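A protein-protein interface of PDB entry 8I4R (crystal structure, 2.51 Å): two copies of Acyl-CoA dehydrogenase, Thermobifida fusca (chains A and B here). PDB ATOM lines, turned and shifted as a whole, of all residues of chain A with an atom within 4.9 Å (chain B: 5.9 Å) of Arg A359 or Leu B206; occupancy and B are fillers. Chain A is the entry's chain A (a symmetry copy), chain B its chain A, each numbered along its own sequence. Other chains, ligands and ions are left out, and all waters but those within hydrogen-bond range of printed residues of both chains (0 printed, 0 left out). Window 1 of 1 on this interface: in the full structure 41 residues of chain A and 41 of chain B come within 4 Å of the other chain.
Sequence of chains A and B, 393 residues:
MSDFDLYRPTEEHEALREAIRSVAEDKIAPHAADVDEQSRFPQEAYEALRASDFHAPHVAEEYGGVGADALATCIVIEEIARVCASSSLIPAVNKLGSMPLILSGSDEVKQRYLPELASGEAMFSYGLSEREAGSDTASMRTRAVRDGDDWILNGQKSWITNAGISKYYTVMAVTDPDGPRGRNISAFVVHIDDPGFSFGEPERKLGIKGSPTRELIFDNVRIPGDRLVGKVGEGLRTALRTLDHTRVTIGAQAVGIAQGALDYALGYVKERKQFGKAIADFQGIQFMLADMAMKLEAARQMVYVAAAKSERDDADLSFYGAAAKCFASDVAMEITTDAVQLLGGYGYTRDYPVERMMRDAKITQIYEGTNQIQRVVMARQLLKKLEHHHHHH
Arg A359 touches just these residues of chain B: Leu B206 (3.6 Å) and Tyr B348 (2.8 Å). Leu B206 touches three residues of chain A. Printed residues of chain A within 4 Å of Lys B362: Tyr A348 (3.96 Å). Of the printed residues of chain B, Lys A362 touches Tyr B348 (3.96 Å). Of the printed residues of chain B, Ile A363 touches Tyr B348 (3.4 Å). The nearest residue of chain B that does not touch Arg A359 is Arg B359 (4.1 Å). The nearest residue of chain A that does not touch Leu B206 is Met A358 (4.5 Å).
Leu A206 touches Tyr B348, and with the chains exchanged Tyr A348 touches Leu B206. Gly A207 touches Tyr B348, and with the chains exchanged Tyr A348 touches Gly B207. Tyr A348 touches Arg B359, and with the chains exchanged Arg A359 touches Tyr B348. Tyr A348 touches Lys B362, and with the chains exchanged Lys A362 touches Tyr B348. Of the 19 pairs that touch across the chains among the printed residues, 12 have their exchanged pair printed and touching as well.
The side-chain amino group (NZ) of Lys B205 lies within hydrogen-bond range of the backbone carbonyl oxygen (O) of Ile B208 (2.9 Å). O of Leu B206 lies within hydrogen-bond range of NH1 of Arg B359 (2.9 Å). The backbone NH (N) of Ile B208 lies within hydrogen-bond range of the side-chain carboxylate (OD1) of Asp B360. NH1 of Arg A359 lies within salt-bridge range of OD1 of Asp A36 (2.8 Å). The guanidinium group of Arg A359 lies within hydrogen-bond range of the backbone carbonyl oxygen of Leu A206 (2.9 Å). The guanidinium group of Arg A359 lies within salt-bridge range of the side-chain carboxylate of Glu A355 (2.9 Å).
O of Arg B204 lies within hydrogen-bond range of N of Arg A350. O of Lys B205 lies within hydrogen-bond range of NH1 of Arg A350. O of Tyr A348 is in hydrogen-bond range of N of Leu B206 (3.0 Å). The backbone NH (N) of Gly B207 sits close to the side-chain hydroxyl (OH) of Tyr A348 (3.2 Å). O of Tyr B348 lies within hydrogen-bond range of N of Leu A206. The side-chain hydroxyl (OH) of Tyr B348 sits close to the backbone NH (N) of Gly A207 (3.2 Å). The side-chain hydroxyl of Tyr B348 sits at hydrogen-bond distance from the backbone carbonyl oxygen of Arg A359 (2.8 Å). The backbone carbonyl oxygen (O) of Arg B359 sits at hydrogen-bond distance from the side-chain hydroxyl (OH) of Tyr A348, at 2.8 Å.
Arg B359 touches Leu A206 (CD to CD1, 3.6 Å). CA of Lys B205 touches O of Tyr A348, 3.4 Å away. OH of Tyr A348 touches N of Ile B208, at 3.7 Å. OH of Tyr A348 touches CA of Asp B360 (3.7 Å). Tyr A348 touches Lys B362 (CE1 to C, 3.96 Å). Arg A350 touches Lys B209. Glu A355 touches Leu B206 (OE2 to CD1, 3.3 Å). Arg A359 touches Leu B206 (CD to CD1, 3.6 Å). C of Lys A362 touches CE1 of Tyr B348, at 3.96 Å. Ile A363 touches Tyr B348 (N to CE1, 3.4 Å).
Of the 12 printed residues of chain B, 10 touch a printed residue of chain A. Printed residues of chain B that touch a printed residue of chain A: Arg B204, Lys B205, Leu B206, Gly B207, Ile B208, Lys B209, Tyr B348, Arg B359, Asp B360 and Lys B362. Hydrophobic or aromatic side chains of chain B that line the printed part of chain A: Leu B206, Ile B208 and Tyr B348. Of the 15 printed residues of chain A, 9 touch a printed residue of chain B. Among the printed residues, no Asp or Glu carboxylate lies within 4 Å of a Lys or Arg side-chain nitrogen of the other chain.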
ATOM      1  N   ASP A  36       8.844  -1.702  -3.190  1.00  0.00           N
ATOM      2  CA  ASP A  36       9.113  -3.057  -2.716  1.00  0.00           C
ATOM      3  C   ASP A  36       7.794  -3.801  -2.401  1.00  0.00           C
ATOM      4  O   ASP A  36       7.530  -4.896  -2.923  1.00  0.00           O
ATOM      5  CB  ASP A  36      10.105  -3.017  -1.527  1.00  0.00           C
ATOM      6  CG  ASP A  36      10.163  -4.337  -0.763  1.00  0.00           C
ATOM      7  OD1 ASP A  36      10.886  -5.272  -1.208  1.00  0.00           O
ATOM      8  OD2 ASP A  36       9.421  -4.446   0.243  1.00  0.00           O
ATOM      9  N   LEU A 206      13.055 -12.297  -3.751  1.00  0.00           N
ATOM     10  CA  LEU A 206      13.426 -11.922  -2.392  1.00  0.00           C
ATOM     11  C   LEU A 206      13.534 -10.402  -2.210  1.00  0.00           C
ATOM     12  O   LEU A 206      13.058  -9.854  -1.219  1.00  0.00           O
ATOM     13  CB  LEU A 206      14.756 -12.632  -2.134  1.00  0.00           C
ATOM     14  CG  LEU A 206      15.462 -12.296  -0.823  1.00  0.00           C
ATOM     15  CD1 LEU A 206      14.592 -12.676   0.373  1.00  0.00           C
ATOM     16  CD2 LEU A 206      16.832 -12.980  -0.743  1.00  0.00           C
ATOM     17  N   GLY A 207      14.247  -9.732  -3.131  1.00  0.00           N
ATOM     18  CA  GLY A 207      14.458  -8.298  -3.115  1.00  0.00           C
ATOM     19  C   GLY A 207      14.522  -7.728  -4.539  1.00  0.00           C
ATOM     20  O   GLY A 207      14.131  -8.415  -5.490  1.00  0.00           O
ATOM     21  N   LYS A 209      12.440  -5.906  -5.645  1.00  0.00           N
ATOM     22  CA  LYS A 209      11.151  -6.367  -6.126  1.00  0.00           C
ATOM     23  C   LYS A 209      10.476  -5.420  -7.122  1.00  0.00           C
ATOM     24  O   LYS A 209       9.685  -5.887  -7.936  1.00  0.00           O
ATOM     25  CB  LYS A 209      10.238  -6.664  -4.948  1.00  0.00           C
ATOM     26  CG  LYS A 209      10.714  -7.828  -4.095  1.00  0.00           C
ATOM     27  CD  LYS A 209       9.907  -8.001  -2.805  1.00  0.00           C
ATOM     28  CE  LYS A 209       8.754  -8.914  -3.056  1.00  0.00           C
ATOM     29  NZ  LYS A 209       7.741  -8.718  -2.032  1.00  0.00           N
ATOM     30  N   TYR A 348      13.010  -6.710  12.059  1.00  0.00           N
ATOM     31  CA  TYR A 348      12.399  -7.843  11.381  1.00  0.00           C
ATOM     32  C   TYR A 348      11.068  -7.473  10.726  1.00  0.00           C
ATOM     33  O   TYR A 348      10.450  -8.360  10.114  1.00  0.00           O
ATOM     34  CB  TYR A 348      12.128  -8.947  12.416  1.00  0.00           C
ATOM     35  CG  TYR A 348      12.078 -10.312  11.813  1.00  0.00           C
ATOM     36  CD1 TYR A 348      13.228 -10.903  11.290  1.00  0.00           C
ATOM     37  CD2 TYR A 348      10.894 -11.026  11.726  1.00  0.00           C
ATOM     38  CE1 TYR A 348      13.189 -12.171  10.707  1.00  0.00           C
ATOM     39  CE2 TYR A 348      10.849 -12.308  11.176  1.00  0.00           C
ATOM     40  CZ  TYR A 348      11.996 -12.882  10.663  1.00  0.00           C
ATOM     41  OH  TYR A 348      11.951 -14.128  10.080  1.00  0.00           O
ATOM     42  N   ARG A 350       8.474  -4.736   8.297  1.00  0.00           N
ATOM     43  CA  ARG A 350       8.523  -3.920   7.070  1.00  0.00           C
ATOM     44  C   ARG A 350       8.234  -2.447   7.368  1.00  0.00           C
ATOM     45  O   ARG A 350       8.377  -1.608   6.494  1.00  0.00           O
ATOM     46  CB  ARG A 350       7.594  -4.405   5.946  1.00  0.00           C
ATOM     47  CG  ARG A 350       7.809  -5.872   5.570  1.00  0.00           C
ATOM     48  CD  ARG A 350       7.594  -6.302   4.111  1.00  0.00           C
ATOM     49  NE  ARG A 350       6.206  -6.545   3.712  1.00  0.00           N
ATOM     50  CZ  ARG A 350       5.437  -7.572   4.093  1.00  0.00           C
ATOM     51  NH1 ARG A 350       5.939  -8.565   4.812  1.00  0.00           N
ATOM     52  NH2 ARG A 350       4.150  -7.598   3.764  1.00  0.00           N
ATOM     53  N   GLU A 355      15.074  -4.494   6.773  1.00  0.00           N
ATOM     54  CA  GLU A 355      14.851  -5.839   6.283  1.00  0.00           C
ATOM     55  C   GLU A 355      14.818  -5.867   4.751  1.00  0.00           C
ATOM     56  O   GLU A 355      15.235  -6.863   4.159  1.00  0.00           O
ATOM     57  CB  GLU A 355      13.629  -6.488   6.946  1.00  0.00           C
ATOM     58  CG  GLU A 355      12.287  -5.870   6.651  1.00  0.00           C
ATOM     59  CD  GLU A 355      11.644  -6.343   5.368  1.00  0.00           C
ATOM     60  OE1 GLU A 355      10.968  -5.500   4.663  1.00  0.00           O
ATOM     61  OE2 GLU A 355      11.815  -7.552   5.083  1.00  0.00           O
ATOM     62  N   ARG A 356      14.265  -4.827   4.105  1.00  0.00           N
ATOM     63  CA  ARG A 356      14.287  -4.746   2.658  1.00  0.00           C
ATOM     64  C   ARG A 356      15.740  -4.608   2.196  1.00  0.00           C
ATOM     65  O   ARG A 356      16.146  -5.166   1.183  1.00  0.00           O
ATOM     66  CB  ARG A 356      13.410  -3.569   2.187  1.00  0.00           C
ATOM     67  CG  ARG A 356      13.547  -3.251   0.703  1.00  0.00           C
ATOM     68  CD  ARG A 356      12.976  -1.941   0.198  1.00  0.00           C
ATOM     69  NE  ARG A 356      13.936  -0.913   0.536  1.00  0.00           N
ATOM     70  CZ  ARG A 356      13.682   0.189   1.233  1.00  0.00           C
ATOM     71  NH1 ARG A 356      12.584   0.359   1.949  1.00  0.00           N
ATOM     72  NH2 ARG A 356      14.586   1.126   1.206  1.00  0.00           N
ATOM     73  N   MET A 357      16.527  -3.833   2.939  1.00  0.00           N
ATOM     74  CA  MET A 357      17.899  -3.563   2.548  1.00  0.00           C
ATOM     75  C   MET A 357      18.701  -4.863   2.600  1.00  0.00           C
ATOM     76  O   MET A 357      19.525  -5.125   1.716  1.00  0.00           O
ATOM     77  CB  MET A 357      18.495  -2.512   3.487  1.00  0.00           C
ATOM     78  CG  MET A 357      18.165  -1.077   3.069  1.00  0.00           C
ATOM     79  SD  MET A 357      18.414   0.057   4.460  1.00  0.00           S
ATOM     80  CE  MET A 357      17.802   1.638   3.878  1.00  0.00           C
ATOM     81  N   MET A 358      18.416  -5.718   3.619  1.00  0.00           N
ATOM     82  CA  MET A 358      19.017  -7.047   3.709  1.00  0.00           C
ATOM     83  C   MET A 358      18.614  -7.931   2.512  1.00  0.00           C
ATOM     84  O   MET A 358      19.457  -8.563   1.862  1.00  0.00           O
ATOM     85  CB  MET A 358      18.663  -7.716   5.036  1.00  0.00           C
ATOM     86  CG  MET A 358      19.257  -9.096   5.166  1.00  0.00           C
ATOM     87  SD  MET A 358      18.768  -9.842   6.717  1.00  0.00           S
ATOM     88  CE  MET A 358      19.326 -11.532   6.481  1.00  0.00           C
ATOM     89  N   ARG A 359      17.323  -7.904   2.169  1.00  0.00           N
ATOM     90  CA  ARG A 359      16.820  -8.683   1.048  1.00  0.00           C
ATOM     91  C   ARG A 359      17.458  -8.227  -0.271  1.00  0.00           C
ATOM     92  O   ARG A 359      17.772  -9.064  -1.108  1.00  0.00           O
ATOM     93  CB  ARG A 359      15.296  -8.585   1.038  1.00  0.00           C
ATOM     94  CG  ARG A 359      14.602  -9.403   2.120  1.00  0.00           C
ATOM     95  CD  ARG A 359      13.070  -9.407   1.961  1.00  0.00           C
ATOM     96  NE  ARG A 359      12.403  -8.131   2.275  1.00  0.00           N
ATOM     97  CZ  ARG A 359      11.790  -7.346   1.390  1.00  0.00           C
ATOM     98  NH1 ARG A 359      11.854  -7.591   0.088  1.00  0.00           N
ATOM     99  NH2 ARG A 359      11.136  -6.284   1.831  1.00  0.00           N
ATOM    100  N   ASP A 360      17.620  -6.907  -0.463  1.00  0.00           N
ATOM    101  CA  ASP A 360      18.199  -6.327  -1.674  1.00  0.00           C
ATOM    102  C   ASP A 360      19.707  -6.604  -1.757  1.00  0.00           C
ATOM    103  O   ASP A 360      20.237  -6.881  -2.832  1.00  0.00           O
ATOM    104  CB  ASP A 360      17.964  -4.817  -1.757  1.00  0.00           C
ATOM    105  CG  ASP A 360      16.516  -4.333  -1.851  1.00  0.00           C
ATOM    106  OD1 ASP A 360      15.552  -5.131  -2.225  1.00  0.00           O
ATOM    107  OD2 ASP A 360      16.348  -3.131  -1.545  1.00  0.00           O
ATOM    108  N   ALA A 361      20.407  -6.588  -0.613  1.00  0.00           N
ATOM    109  CA  ALA A 361      21.848  -6.811  -0.606  1.00  0.00           C
ATOM    110  C   ALA A 361      22.228  -8.181  -1.185  1.00  0.00           C
ATOM    111  O   ALA A 361      23.254  -8.315  -1.889  1.00  0.00           O
ATOM    112  CB  ALA A 361      22.362  -6.647   0.795  1.00  0.00           C
ATOM    113  N   LYS A 362      21.386  -9.195  -0.911  1.00  0.00           N
ATOM    114  CA  LYS A 362      21.678 -10.556  -1.323  1.00  0.00           C
ATOM    115  C   LYS A 362      21.812 -10.688  -2.839  1.00  0.00           C
ATOM    116  O   LYS A 362      22.603 -11.504  -3.286  1.00  0.00           O
ATOM    117  CB  LYS A 362      20.614 -11.522  -0.797  1.00  0.00           C
ATOM    118  CG  LYS A 362      20.819 -12.990  -1.172  1.00  0.00           C
ATOM    119  CD  LYS A 362      22.052 -13.592  -0.568  1.00  0.00           C
ATOM    120  CE  LYS A 362      22.771 -14.519  -1.512  1.00  0.00           C
ATOM    121  NZ  LYS A 362      24.015 -15.063  -0.923  1.00  0.00           N
ATOM    122  N   ILE A 363      21.076  -9.897  -3.640  1.00  0.00           N
ATOM    123  CA  ILE A 363      21.209  -9.990  -5.089  1.00  0.00           C
ATOM    124  C   ILE A 363      22.620  -9.593  -5.527  1.00  0.00           C
ATOM    125  O   ILE A 363      23.079 -10.094  -6.538  1.00  0.00           O
ATOM    126  CB  ILE A 363      20.168  -9.170  -5.897  1.00  0.00           C
ATOM    127  CG1 ILE A 363      20.180  -9.577  -7.381  1.00  0.00           C
ATOM    128  CG2 ILE A 363      20.360  -7.658  -5.796  1.00  0.00           C
ATOM    129  CD1 ILE A 363      19.811 -11.059  -7.658  1.00  0.00           C
ATOM    130  N   ASP B  36       3.757 -18.957   3.912  1.00  0.00           N
ATOM    131  CA  ASP B  36       4.620 -17.784   3.808  1.00  0.00           C
ATOM    132  C   ASP B  36       4.002 -16.730   2.860  1.00  0.00           C
ATOM    133  O   ASP B  36       3.808 -15.562   3.231  1.00  0.00           O
ATOM    134  CB  ASP B  36       6.055 -18.213   3.414  1.00  0.00           C
ATOM    135  CG  ASP B  36       6.914 -17.039   2.950  1.00  0.00           C
ATOM    136  OD1 ASP B  36       7.476 -16.310   3.815  1.00  0.00           O
ATOM    137  OD2 ASP B  36       6.958 -16.818   1.715  1.00  0.00           O
ATOM    138  N   ARG B 204       3.830  -6.932   9.790  1.00  0.00           N
ATOM    139  CA  ARG B 204       4.354  -7.366   8.498  1.00  0.00           C
ATOM    140  C   ARG B 204       5.847  -7.677   8.693  1.00  0.00           C
ATOM    141  O   ARG B 204       6.618  -6.843   9.151  1.00  0.00           O
ATOM    142  CB  ARG B 204       4.071  -6.277   7.453  1.00  0.00           C
ATOM    143  CG  ARG B 204       2.606  -5.910   7.214  1.00  0.00           C
ATOM    144  CD  ARG B 204       2.386  -4.391   7.144  1.00  0.00           C
ATOM    145  NE  ARG B 204       2.904  -3.778   5.917  1.00  0.00           N
ATOM    146  CZ  ARG B 204       3.837  -2.807   5.824  1.00  0.00           C
ATOM    147  NH1 ARG B 204       4.168  -2.043   6.858  1.00  0.00           N
ATOM    148  NH2 ARG B 204       4.435  -2.602   4.656  1.00  0.00           N
ATOM    149  N   LYS B 205       6.238  -8.929   8.464  1.00  0.00           N
ATOM    150  CA  LYS B 205       7.550  -9.452   8.827  1.00  0.00           C
ATOM    151  C   LYS B 205       8.327  -9.900   7.593  1.00  0.00           C
ATOM    152  O   LYS B 205       7.725 -10.263   6.574  1.00  0.00           O
ATOM    153  CB  LYS B 205       7.417 -10.656   9.766  1.00  0.00           C
ATOM    154  CG  LYS B 205       6.531 -10.335  10.960  1.00  0.00           C
ATOM    155  CD  LYS B 205       6.761 -11.147  12.162  1.00  0.00           C
ATOM    156  CE  LYS B 205       6.675 -12.635  11.920  1.00  0.00           C
ATOM    157  NZ  LYS B 205       5.289 -13.058  11.690  1.00  0.00           N
ATOM    158  N   LEU B 206       9.653  -9.982   7.780  1.00  0.00           N
ATOM    159  CA  LEU B 206      10.616 -10.570   6.858  1.00  0.00           C
ATOM    160  C   LEU B 206      10.374 -12.068   6.632  1.00  0.00           C
ATOM    161  O   LEU B 206      10.427 -12.548   5.502  1.00  0.00           O
ATOM    162  CB  LEU B 206      11.985 -10.292   7.482  1.00  0.00           C
ATOM    163  CG  LEU B 206      13.187 -10.933   6.796  1.00  0.00           C
ATOM    164  CD1 LEU B 206      13.320 -10.436   5.358  1.00  0.00           C
ATOM    165  CD2 LEU B 206      14.476 -10.676   7.585  1.00  0.00           C
ATOM    166  N   GLY B 207      10.198 -12.825   7.728  1.00  0.00           N
ATOM    167  CA  GLY B 207       9.964 -14.255   7.705  1.00  0.00           C
ATOM    168  C   GLY B 207       9.029 -14.685   8.844  1.00  0.00           C
ATOM    169  O   GLY B 207       8.375 -13.831   9.453  1.00  0.00           O
ATOM    170  N   ILE B 208       8.981 -16.028   9.051  1.00  0.00           N
ATOM    171  CA  ILE B 208       7.957 -16.751   9.776  1.00  0.00           C
ATOM    172  C   ILE B 208       6.643 -15.993   9.624  1.00  0.00           C
ATOM    173  O   ILE B 208       5.964 -15.671  10.594  1.00  0.00           O
ATOM    174  CB  ILE B 208       8.374 -17.020  11.241  1.00  0.00           C
ATOM    175  CG1 ILE B 208       8.844 -15.767  11.976  1.00  0.00           C
ATOM    176  CG2 ILE B 208       9.418 -18.115  11.336  1.00  0.00           C
ATOM    177  CD1 ILE B 208       8.516 -15.766  13.476  1.00  0.00           C
ATOM    178  N   LYS B 209       6.281 -15.734   8.369  1.00  0.00           N
ATOM    179  CA  LYS B 209       5.146 -14.884   8.057  1.00  0.00           C
ATOM    180  C   LYS B 209       3.786 -15.506   8.387  1.00  0.00           C
ATOM    181  O   LYS B 209       2.842 -14.760   8.634  1.00  0.00           O
ATOM    182  CB  LYS B 209       5.212 -14.451   6.602  1.00  0.00           C
ATOM    183  CG  LYS B 209       6.398 -13.554   6.293  1.00  0.00           C
ATOM    184  CD  LYS B 209       6.574 -13.280   4.797  1.00  0.00           C
ATOM    185  CE  LYS B 209       5.805 -12.059   4.418  1.00  0.00           C
ATOM    186  NZ  LYS B 209       5.566 -12.055   2.985  1.00  0.00           N
ATOM    187  N   TYR B 348      17.172 -16.765  -5.585  1.00  0.00           N
ATOM    188  CA  TYR B 348      16.633 -15.448  -5.283  1.00  0.00           C
ATOM    189  C   TYR B 348      15.131 -15.364  -5.555  1.00  0.00           C
ATOM    190  O   TYR B 348      14.555 -14.286  -5.334  1.00  0.00           O
ATOM    191  CB  TYR B 348      17.336 -14.413  -6.176  1.00  0.00           C
ATOM    192  CG  TYR B 348      17.336 -13.040  -5.591  1.00  0.00           C
ATOM    193  CD1 TYR B 348      18.080 -12.752  -4.447  1.00  0.00           C
ATOM    194  CD2 TYR B 348      16.580 -12.016  -6.138  1.00  0.00           C
ATOM    195  CE1 TYR B 348      18.072 -11.477  -3.880  1.00  0.00           C
ATOM    196  CE2 TYR B 348      16.590 -10.728  -5.599  1.00  0.00           C
ATOM    197  CZ  TYR B 348      17.335 -10.457  -4.467  1.00  0.00           C
ATOM    198  OH  TYR B 348      17.316  -9.201  -3.905  1.00  0.00           O
ATOM    199  N   MET B 358      16.155 -18.460   4.291  1.00  0.00           N
ATOM    200  CA  MET B 358      17.043 -17.370   4.688  1.00  0.00           C
ATOM    201  C   MET B 358      16.294 -16.301   5.508  1.00  0.00           C
ATOM    202  O   MET B 358      16.742 -15.876   6.580  1.00  0.00           O
ATOM    203  CB  MET B 358      17.728 -16.753   3.470  1.00  0.00           C
ATOM    204  CG  MET B 358      18.649 -15.616   3.835  1.00  0.00           C
ATOM    205  SD  MET B 358      19.381 -14.909   2.363  1.00  0.00           S
ATOM    206  CE  MET B 358      20.149 -13.431   3.033  1.00  0.00           C
ATOM    207  N   ARG B 359      15.099 -15.929   5.039  1.00  0.00           N
ATOM    208  CA  ARG B 359      14.287 -14.940   5.729  1.00  0.00           C
ATOM    209  C   ARG B 359      13.884 -15.434   7.125  1.00  0.00           C
ATOM    210  O   ARG B 359      13.878 -14.646   8.062  1.00  0.00           O
ATOM    211  CB  ARG B 359      13.086 -14.602   4.847  1.00  0.00           C
ATOM    212  CG  ARG B 359      13.412 -13.725   3.644  1.00  0.00           C
ATOM    213  CD  ARG B 359      12.147 -13.273   2.889  1.00  0.00           C
ATOM    214  NE  ARG B 359      11.457 -14.332   2.131  1.00  0.00           N
ATOM    215  CZ  ARG B 359      10.255 -14.826   2.422  1.00  0.00           C
ATOM    216  NH1 ARG B 359       9.621 -14.490   3.537  1.00  0.00           N
ATOM    217  NH2 ARG B 359       9.708 -15.696   1.588  1.00  0.00           N
ATOM    218  N   ASP B 360      13.524 -16.722   7.252  1.00  0.00           N
ATOM    219  CA  ASP B 360      13.104 -17.327   8.515  1.00  0.00           C
ATOM    220  C   ASP B 360      14.289 -17.482   9.478  1.00  0.00           C
ATOM    221  O   ASP B 360      14.152 -17.268  10.682  1.00  0.00           O
ATOM    222  CB  ASP B 360      12.449 -18.695   8.306  1.00  0.00           C
ATOM    223  CG  ASP B 360      11.148 -18.739   7.502  1.00  0.00           C
ATOM    224  OD1 ASP B 360      10.421 -17.670   7.322  1.00  0.00           O
ATOM    225  OD2 ASP B 360      10.858 -19.867   7.045  1.00  0.00           O
ATOM    226  N   LYS B 362      16.796 -15.561  10.003  1.00  0.00           N
ATOM    227  CA  LYS B 362      17.166 -14.307  10.631  1.00  0.00           C
ATOM    228  C   LYS B 362      16.430 -14.078  11.950  1.00  0.00           C
ATOM    229  O   LYS B 362      17.009 -13.482  12.845  1.00  0.00           O
ATOM    230  CB  LYS B 362      16.929 -13.132   9.679  1.00  0.00           C
ATOM    231  CG  LYS B 362      17.284 -11.754  10.238  1.00  0.00           C
ATOM    232  CD  LYS B 362      18.747 -11.583  10.516  1.00  0.00           C
ATOM    233  CE  LYS B 362      19.014 -10.815  11.783  1.00  0.00           C
ATOM    234  NZ  LYS B 362      20.461 -10.701  12.074  1.00  0.00           N
